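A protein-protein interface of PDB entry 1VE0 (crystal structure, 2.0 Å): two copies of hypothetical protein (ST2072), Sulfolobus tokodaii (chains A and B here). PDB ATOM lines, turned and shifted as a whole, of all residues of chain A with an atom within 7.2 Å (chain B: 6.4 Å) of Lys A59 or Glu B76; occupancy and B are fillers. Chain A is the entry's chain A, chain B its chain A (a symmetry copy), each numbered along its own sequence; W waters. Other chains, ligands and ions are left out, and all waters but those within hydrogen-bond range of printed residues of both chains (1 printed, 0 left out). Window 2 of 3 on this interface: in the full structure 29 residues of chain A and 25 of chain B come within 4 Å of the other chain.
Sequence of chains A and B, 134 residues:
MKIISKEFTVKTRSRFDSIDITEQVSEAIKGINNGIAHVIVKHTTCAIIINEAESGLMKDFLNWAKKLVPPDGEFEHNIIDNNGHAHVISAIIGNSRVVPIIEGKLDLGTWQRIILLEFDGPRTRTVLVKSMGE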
ATOM      1  N   SER A  18      -8.102   4.949  18.895  1.00  0.00           N
ATOM      2  CA  SER A  18      -6.724   5.385  19.083  1.00  0.00           C
ATOM      3  C   SER A  18      -6.593   6.747  18.416  1.00  0.00           C
ATOM      4  O   SER A  18      -6.950   6.926  17.255  1.00  0.00           O
ATOM      5  CB  SER A  18      -5.743   4.366  18.491  1.00  0.00           C
ATOM      6  OG  SER A  18      -6.135   3.940  17.200  1.00  0.00           O
ATOM      7  N   GLU A  54       1.169   4.785  12.574  1.00  0.00           N
ATOM      8  CA  GLU A  54       0.894   4.323  11.223  1.00  0.00           C
ATOM      9  C   GLU A  54      -0.535   3.767  11.226  1.00  0.00           C
ATOM     10  O   GLU A  54      -0.991   3.193  12.220  1.00  0.00           O
ATOM     11  CB  GLU A  54       1.892   3.243  10.798  1.00  0.00           C
ATOM     12  CG  GLU A  54       1.681   2.766   9.362  1.00  0.00           C
ATOM     13  CD  GLU A  54       0.800   1.535   9.278  1.00  0.00           C
ATOM     14  OE1 GLU A  54       0.031   1.416   8.295  1.00  0.00           O
ATOM     15  OE2 GLU A  54       0.891   0.677  10.186  1.00  0.00           O
ATOM     16  N   SER A  55      -1.244   3.948  10.117  1.00  0.00           N
ATOM     17  CA  SER A  55      -2.626   3.491  10.010  1.00  0.00           C
ATOM     18  C   SER A  55      -2.926   2.078  10.517  1.00  0.00           C
ATOM     19  O   SER A  55      -3.830   1.890  11.335  1.00  0.00           O
ATOM     20  CB  SER A  55      -3.103   3.604   8.563  1.00  0.00           C
ATOM     21  OG  SER A  55      -4.408   3.074   8.457  1.00  0.00           O
ATOM     22  N   GLY A  56      -2.184   1.088  10.028  1.00  0.00           N
ATOM     23  CA  GLY A  56      -2.422  -0.283  10.446  1.00  0.00           C
ATOM     24  C   GLY A  56      -2.144  -0.504  11.921  1.00  0.00           C
ATOM     25  O   GLY A  56      -2.926  -1.139  12.636  1.00  0.00           O
ATOM     26  N   LEU A  57      -1.021   0.044  12.374  1.00  0.00           N
ATOM     27  CA  LEU A  57      -0.594  -0.079  13.760  1.00  0.00           C
ATOM     28  C   LEU A  57      -1.632   0.545  14.705  1.00  0.00           C
ATOM     29  O   LEU A  57      -1.878   0.034  15.792  1.00  0.00           O
ATOM     30  CB  LEU A  57       0.771   0.598  13.902  1.00  0.00           C
ATOM     31  CG  LEU A  57       1.797   0.100  14.910  1.00  0.00           C
ATOM     32  CD1 LEU A  57       2.013  -1.404  14.778  1.00  0.00           C
ATOM     33  CD2 LEU A  57       3.102   0.863  14.674  1.00  0.00           C
ATOM     34  N   MET A  58      -2.258   1.638  14.285  1.00  0.00           N
ATOM     35  CA  MET A  58      -3.262   2.278  15.126  1.00  0.00           C
ATOM     36  C   MET A  58      -4.401   1.296  15.399  1.00  0.00           C
ATOM     37  O   MET A  58      -5.070   1.386  16.426  1.00  0.00           O
ATOM     38  CB  MET A  58      -3.774   3.556  14.462  1.00  0.00           C
ATOM     39  CG  MET A  58      -2.764   4.693  14.488  1.00  0.00           C
ATOM     40  SD  MET A  58      -2.368   5.278  16.324  1.00  0.00           S
ATOM     41  CE  MET A  58      -3.725   6.673  16.418  1.00  0.00           C
ATOM     42  N   LYS A  59      -4.606   0.348  14.485  1.00  0.00           N
ATOM     43  CA  LYS A  59      -5.630  -0.676  14.668  1.00  0.00           C
ATOM     44  C   LYS A  59      -5.045  -1.809  15.529  1.00  0.00           C
ATOM     45  O   LYS A  59      -5.697  -2.303  16.448  1.00  0.00           O
ATOM     46  CB  LYS A  59      -6.073  -1.258  13.320  1.00  0.00           C
ATOM     47  CG  LYS A  59      -6.865  -0.325  12.417  1.00  0.00           C
ATOM     48  CD  LYS A  59      -7.309  -1.102  11.183  1.00  0.00           C
ATOM     49  CE  LYS A  59      -8.163  -0.281  10.235  1.00  0.00           C
ATOM     50  NZ  LYS A  59      -7.363   0.680   9.436  1.00  0.00           N
ATOM     51  N   ASP A  60      -3.818  -2.219  15.207  1.00  0.00           N
ATOM     52  CA  ASP A  60      -3.119  -3.281  15.938  1.00  0.00           C
ATOM     53  C   ASP A  60      -3.084  -3.072  17.462  1.00  0.00           C
ATOM     54  O   ASP A  60      -3.295  -4.020  18.223  1.00  0.00           O
ATOM     55  CB  ASP A  60      -1.671  -3.405  15.438  1.00  0.00           C
ATOM     56  CG  ASP A  60      -1.574  -3.951  14.020  1.00  0.00           C
ATOM     57  OD1 ASP A  60      -0.548  -3.675  13.347  1.00  0.00           O
ATOM     58  OD2 ASP A  60      -2.507  -4.662  13.582  1.00  0.00           O
ATOM     59  N   PHE A  61      -2.804  -1.849  17.914  1.00  0.00           N
ATOM     60  CA  PHE A  61      -2.740  -1.603  19.356  1.00  0.00           C
ATOM     61  C   PHE A  61      -4.047  -2.025  20.022  1.00  0.00           C
ATOM     62  O   PHE A  61      -4.040  -2.673  21.068  1.00  0.00           O
ATOM     63  CB  PHE A  61      -2.479  -0.117  19.679  1.00  0.00           C
ATOM     64  CG  PHE A  61      -1.149   0.395  19.203  1.00  0.00           C
ATOM     65  CD1 PHE A  61       0.026  -0.313  19.464  1.00  0.00           C
ATOM     66  CD2 PHE A  61      -1.072   1.573  18.462  1.00  0.00           C
ATOM     67  CE1 PHE A  61       1.258   0.143  18.990  1.00  0.00           C
ATOM     68  CE2 PHE A  61       0.153   2.034  17.984  1.00  0.00           C
ATOM     69  CZ  PHE A  61       1.324   1.315  18.249  1.00  0.00           C
ATOM     70  N   LEU A  62      -5.161  -1.646  19.400  1.00  0.00           N
ATOM     71  CA  LEU A  62      -6.489  -1.955  19.911  1.00  0.00           C
ATOM     72  C   LEU A  62      -6.819  -3.438  19.789  1.00  0.00           C
ATOM     73  O   LEU A  62      -7.283  -4.053  20.747  1.00  0.00           O
ATOM     74  CB  LEU A  62      -7.534  -1.123  19.167  1.00  0.00           C
ATOM     75  CG  LEU A  62      -7.239   0.378  19.230  1.00  0.00           C
ATOM     76  CD1 LEU A  62      -8.247   1.135  18.380  1.00  0.00           C
ATOM     77  CD2 LEU A  62      -7.284   0.833  20.684  1.00  0.00           C
ATOM     78  N   ASN A  63      -6.571  -4.015  18.620  1.00  0.00           N
ATOM     79  CA  ASN A  63      -6.854  -5.431  18.421  1.00  0.00           C
ATOM     80  C   ASN A  63      -6.018  -6.344  19.309  1.00  0.00           C
ATOM     81  O   ASN A  63      -6.495  -7.386  19.765  1.00  0.00           O
ATOM     82  CB  ASN A  63      -6.672  -5.815  16.948  1.00  0.00           C
ATOM     83  CG  ASN A  63      -7.718  -5.179  16.061  1.00  0.00           C
ATOM     84  OD1 ASN A  63      -8.874  -5.029  16.467  1.00  0.00           O
ATOM     85  ND2 ASN A  63      -7.330  -4.815  14.841  1.00  0.00           N
ATOM     86  N   TRP A  64      -4.770  -5.973  19.569  1.00  0.00           N
ATOM     87  CA  TRP A  64      -3.955  -6.812  20.433  1.00  0.00           C
ATOM     88  C   TRP A  64      -4.319  -6.586  21.888  1.00  0.00           C
ATOM     89  O   TRP A  64      -4.198  -7.486  22.715  1.00  0.00           O
ATOM     90  CB  TRP A  64      -2.470  -6.578  20.171  1.00  0.00           C
ATOM     91  CG  TRP A  64      -2.043  -7.381  18.999  1.00  0.00           C
ATOM     92  CD1 TRP A  64      -2.116  -7.021  17.682  1.00  0.00           C
ATOM     93  CD2 TRP A  64      -1.647  -8.756  19.018  1.00  0.00           C
ATOM     94  NE1 TRP A  64      -1.796  -8.096  16.878  1.00  0.00           N
ATOM     95  CE2 TRP A  64      -1.507  -9.172  17.674  1.00  0.00           C
ATOM     96  CE3 TRP A  64      -1.402  -9.681  20.044  1.00  0.00           C
ATOM     97  CZ2 TRP A  64      -1.136 -10.473  17.330  1.00  0.00           C
ATOM     98  CZ3 TRP A  64      -1.030 -10.976  19.700  1.00  0.00           C
ATOM     99  CH2 TRP A  64      -0.903 -11.359  18.354  1.00  0.00           C
ATOM    100  N   ALA A  65      -4.790  -5.384  22.198  1.00  0.00           N
ATOM    101  CA  ALA A  65      -5.218  -5.106  23.557  1.00  0.00           C
ATOM    102  C   ALA A  65      -6.402  -6.043  23.789  1.00  0.00           C
ATOM    103  O   ALA A  65      -6.512  -6.686  24.835  1.00  0.00           O
ATOM    104  CB  ALA A  65      -5.659  -3.657  23.686  1.00  0.00           C
ATOM    105  N   LYS A  66      -7.284  -6.124  22.796  1.00  0.00           N
ATOM    106  CA  LYS A  66      -8.452  -6.997  22.898  1.00  0.00           C
ATOM    107  C   LYS A  66      -8.052  -8.464  23.018  1.00  0.00           C
ATOM    108  O   LYS A  66      -8.729  -9.239  23.695  1.00  0.00           O
ATOM    109  CB  LYS A  66      -9.377  -6.819  21.686  1.00  0.00           C
ATOM    110  CG  LYS A  66     -10.180  -5.533  21.725  1.00  0.00           C
ATOM    111  CD  LYS A  66     -11.357  -5.542  20.750  1.00  0.00           C
ATOM    112  CE  LYS A  66     -10.894  -5.539  19.314  1.00  0.00           C
ATOM    113  NZ  LYS A  66     -12.030  -5.343  18.372  1.00  0.00           N
ATOM    114  N   GLU B  74      -0.889 -11.753  13.619  1.00  0.00           N
ATOM    115  CA  GLU B  74      -1.535 -10.928  12.609  1.00  0.00           C
ATOM    116  C   GLU B  74      -1.416  -9.448  12.970  1.00  0.00           C
ATOM    117  O   GLU B  74      -1.895  -9.025  14.020  1.00  0.00           O
ATOM    118  CB  GLU B  74      -3.009 -11.329  12.495  1.00  0.00           C
ATOM    119  CG  GLU B  74      -3.839 -10.431  11.604  1.00  0.00           C
ATOM    120  CD  GLU B  74      -5.302 -10.842  11.563  1.00  0.00           C
ATOM    121  OE1 GLU B  74      -6.105 -10.124  10.923  1.00  0.00           O
ATOM    122  OE2 GLU B  74      -5.648 -11.884  12.167  1.00  0.00           O
ATOM    123  N   PHE B  75      -0.766  -8.676  12.100  1.00  0.00           N
ATOM    124  CA  PHE B  75      -0.563  -7.237  12.305  1.00  0.00           C
ATOM    125  C   PHE B  75      -0.812  -6.464  11.008  1.00  0.00           C
ATOM    126  O   PHE B  75      -0.171  -6.725   9.989  1.00  0.00           O
ATOM    127  CB  PHE B  75       0.875  -6.961  12.766  1.00  0.00           C
ATOM    128  CG  PHE B  75       1.240  -7.623  14.067  1.00  0.00           C
ATOM    129  CD1 PHE B  75       0.826  -7.078  15.287  1.00  0.00           C
ATOM    130  CD2 PHE B  75       1.982  -8.796  14.076  1.00  0.00           C
ATOM    131  CE1 PHE B  75       1.150  -7.696  16.492  1.00  0.00           C
ATOM    132  CE2 PHE B  75       2.311  -9.425  15.277  1.00  0.00           C
ATOM    133  CZ  PHE B  75       1.893  -8.874  16.490  1.00  0.00           C
ATOM    134  N   GLU B  76      -1.729  -5.505  11.036  1.00  0.00           N
ATOM    135  CA  GLU B  76      -2.001  -4.728   9.836  1.00  0.00           C
ATOM    136  C   GLU B  76      -0.778  -3.925   9.421  1.00  0.00           C
ATOM    137  O   GLU B  76      -0.599  -3.588   8.244  1.00  0.00           O
ATOM    138  CB  GLU B  76      -3.182  -3.794  10.068  1.00  0.00           C
ATOM    139  CG  GLU B  76      -4.472  -4.538  10.324  1.00  0.00           C
ATOM    140  CD  GLU B  76      -5.669  -3.849   9.703  1.00  0.00           C
ATOM    141  OE1 GLU B  76      -6.781  -4.424   9.772  1.00  0.00           O
ATOM    142  OE2 GLU B  76      -5.498  -2.737   9.144  1.00  0.00           O
ATOM    143  N   HIS B  77       0.069  -3.623  10.399  1.00  0.00           N
ATOM    144  CA  HIS B  77       1.278  -2.861  10.139  1.00  0.00           C
ATOM    145  C   HIS B  77       2.240  -3.626   9.243  1.00  0.00           C
ATOM    146  O   HIS B  77       2.969  -3.025   8.451  1.00  0.00           O
ATOM    147  CB  HIS B  77       1.989  -2.541  11.453  1.00  0.00           C
ATOM    148  CG  HIS B  77       3.279  -1.810  11.276  1.00  0.00           C
ATOM    149  ND1 HIS B  77       3.341  -0.508  10.833  1.00  0.00           N
ATOM    150  CD2 HIS B  77       4.561  -2.205  11.468  1.00  0.00           C
ATOM    151  CE1 HIS B  77       4.605  -0.130  10.758  1.00  0.00           C
ATOM    152  NE2 HIS B  77       5.365  -1.142  11.138  1.00  0.00           N
ATOM    153  N   ASN B  78       2.237  -4.950   9.368  1.00  0.00           N
ATOM    154  CA  ASN B  78       3.159  -5.778   8.599  1.00  0.00           C
ATOM    155  C   ASN B  78       3.000  -5.704   7.090  1.00  0.00           C
ATOM    156  O   ASN B  78       3.766  -6.321   6.351  1.00  0.00           O
ATOM    157  CB  ASN B  78       3.116  -7.224   9.110  1.00  0.00           C
ATOM    158  CG  ASN B  78       3.801  -7.373  10.474  1.00  0.00           C
ATOM    159  OD1 ASN B  78       4.074  -6.383  11.147  1.00  0.00           O
ATOM    160  ND2 ASN B  78       4.072  -8.604  10.879  1.00  0.00           N
ATOM    161  N   ILE B  79       2.016  -4.933   6.637  1.00  0.00           N
ATOM    162  CA  ILE B  79       1.796  -4.716   5.211  1.00  0.00           C
ATOM    163  C   ILE B  79       2.932  -3.796   4.764  1.00  0.00           C
ATOM    164  O   ILE B  79       3.373  -3.836   3.618  1.00  0.00           O
ATOM    165  CB  ILE B  79       0.452  -3.988   4.948  1.00  0.00           C
ATOM    166  CG1 ILE B  79      -0.717  -4.958   5.128  1.00  0.00           C
ATOM    167  CG2 ILE B  79       0.443  -3.382   3.553  1.00  0.00           C
ATOM    168  CD1 ILE B  79      -2.079  -4.292   5.060  1.00  0.00           C
ATOM    169  N   ILE B  80       3.397  -2.969   5.692  1.00  0.00           N
ATOM    170  CA  ILE B  80       4.470  -2.019   5.425  1.00  0.00           C
ATOM    171  C   ILE B  80       5.839  -2.487   5.909  1.00  0.00           C
ATOM    172  O   ILE B  80       6.840  -2.289   5.232  1.00  0.00           O
ATOM    173  CB  ILE B  80       4.186  -0.665   6.105  1.00  0.00           C
ATOM    174  CG1 ILE B  80       2.865  -0.089   5.594  1.00  0.00           C
ATOM    175  CG2 ILE B  80       5.340   0.301   5.839  1.00  0.00           C
ATOM    176  CD1 ILE B  80       2.502   1.239   6.212  1.00  0.00           C
HETATM  177  O   HOH W   1      -0.652  -0.990   7.173  1.00  0.00           O
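ND1 of His B77 is in hydrogen-bond range of OE2 of Glu A54 (2.8 Å).
The side-chain amino group (NZ) of Lys A59 lies within salt-bridge range of the side-chain carboxylate (OE2) of Glu B76 (3.9 Å).
OD2 of Asp A60 lies within hydrogen-bond range of N of Glu B76.
The side-chain carboxylate (OD1) of Asp A60 lies within hydrogen-bond range of the backbone NH (N) of His B77.
The backbone carbonyl oxygen (O) of Glu B74 lies within hydrogen-bond range of the indole nitrogen (NE1) of Trp A64 (3.0 Å).
Among the printed residues, pairs that only touch across the chains: Glu A54 with Ile B80, Gly A56 with Glu B76, Leu A57 with His B77, Asp A60 with Phe B75 and Trp A64 with Phe B75.
Glu B76 touches just these residues of chain A: Gly A56 (3.6 Å), Lys A59 (3.2 Å) and Asp A60 (2.8 Å).
Printed residues of chain A within 4 Å of His B77: Glu A54, Leu A57 and Asp A60.
Of the printed residues of chain B, Trp A64 touches Glu B74 (3.0 Å) and Phe B75 (3.0 Å).
Of the printed residues of chain B, Glu A54 touches His B77 and Ile B80.
Of the printed residues of chain A, Ile B80 touches Glu A54 (3.2 Å).
Printed residues of chain B within 4 Å of Leu A57: His B77 (3.5 Å).
Water W1 lies within hydrogen-bond range of the side-chain carboxylate (OE1) of Glu A54 and the backbone carbonyl oxygen (O) of Glu B76.
No position is printed for both chains.
The side-chain carboxylate of Glu A54 is in hydrogen-bond range of the backbone NH of Gly A56 (2.8 Å).
The side-chain carboxylate (OE2) of Glu A54 lies within hydrogen-bond range of the backbone NH (N) of Leu A57 (3.0 Å).
ND2 of Asn A63 sits at hydrogen-bond distance from O of Lys A59 (3.4 Å).
Among the printed residues, Asp or Glu carboxylates within 4 Å of a Lys or Arg side-chain nitrogen of the other chain: Lys A59 with Glu B76 (3.9 Å).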
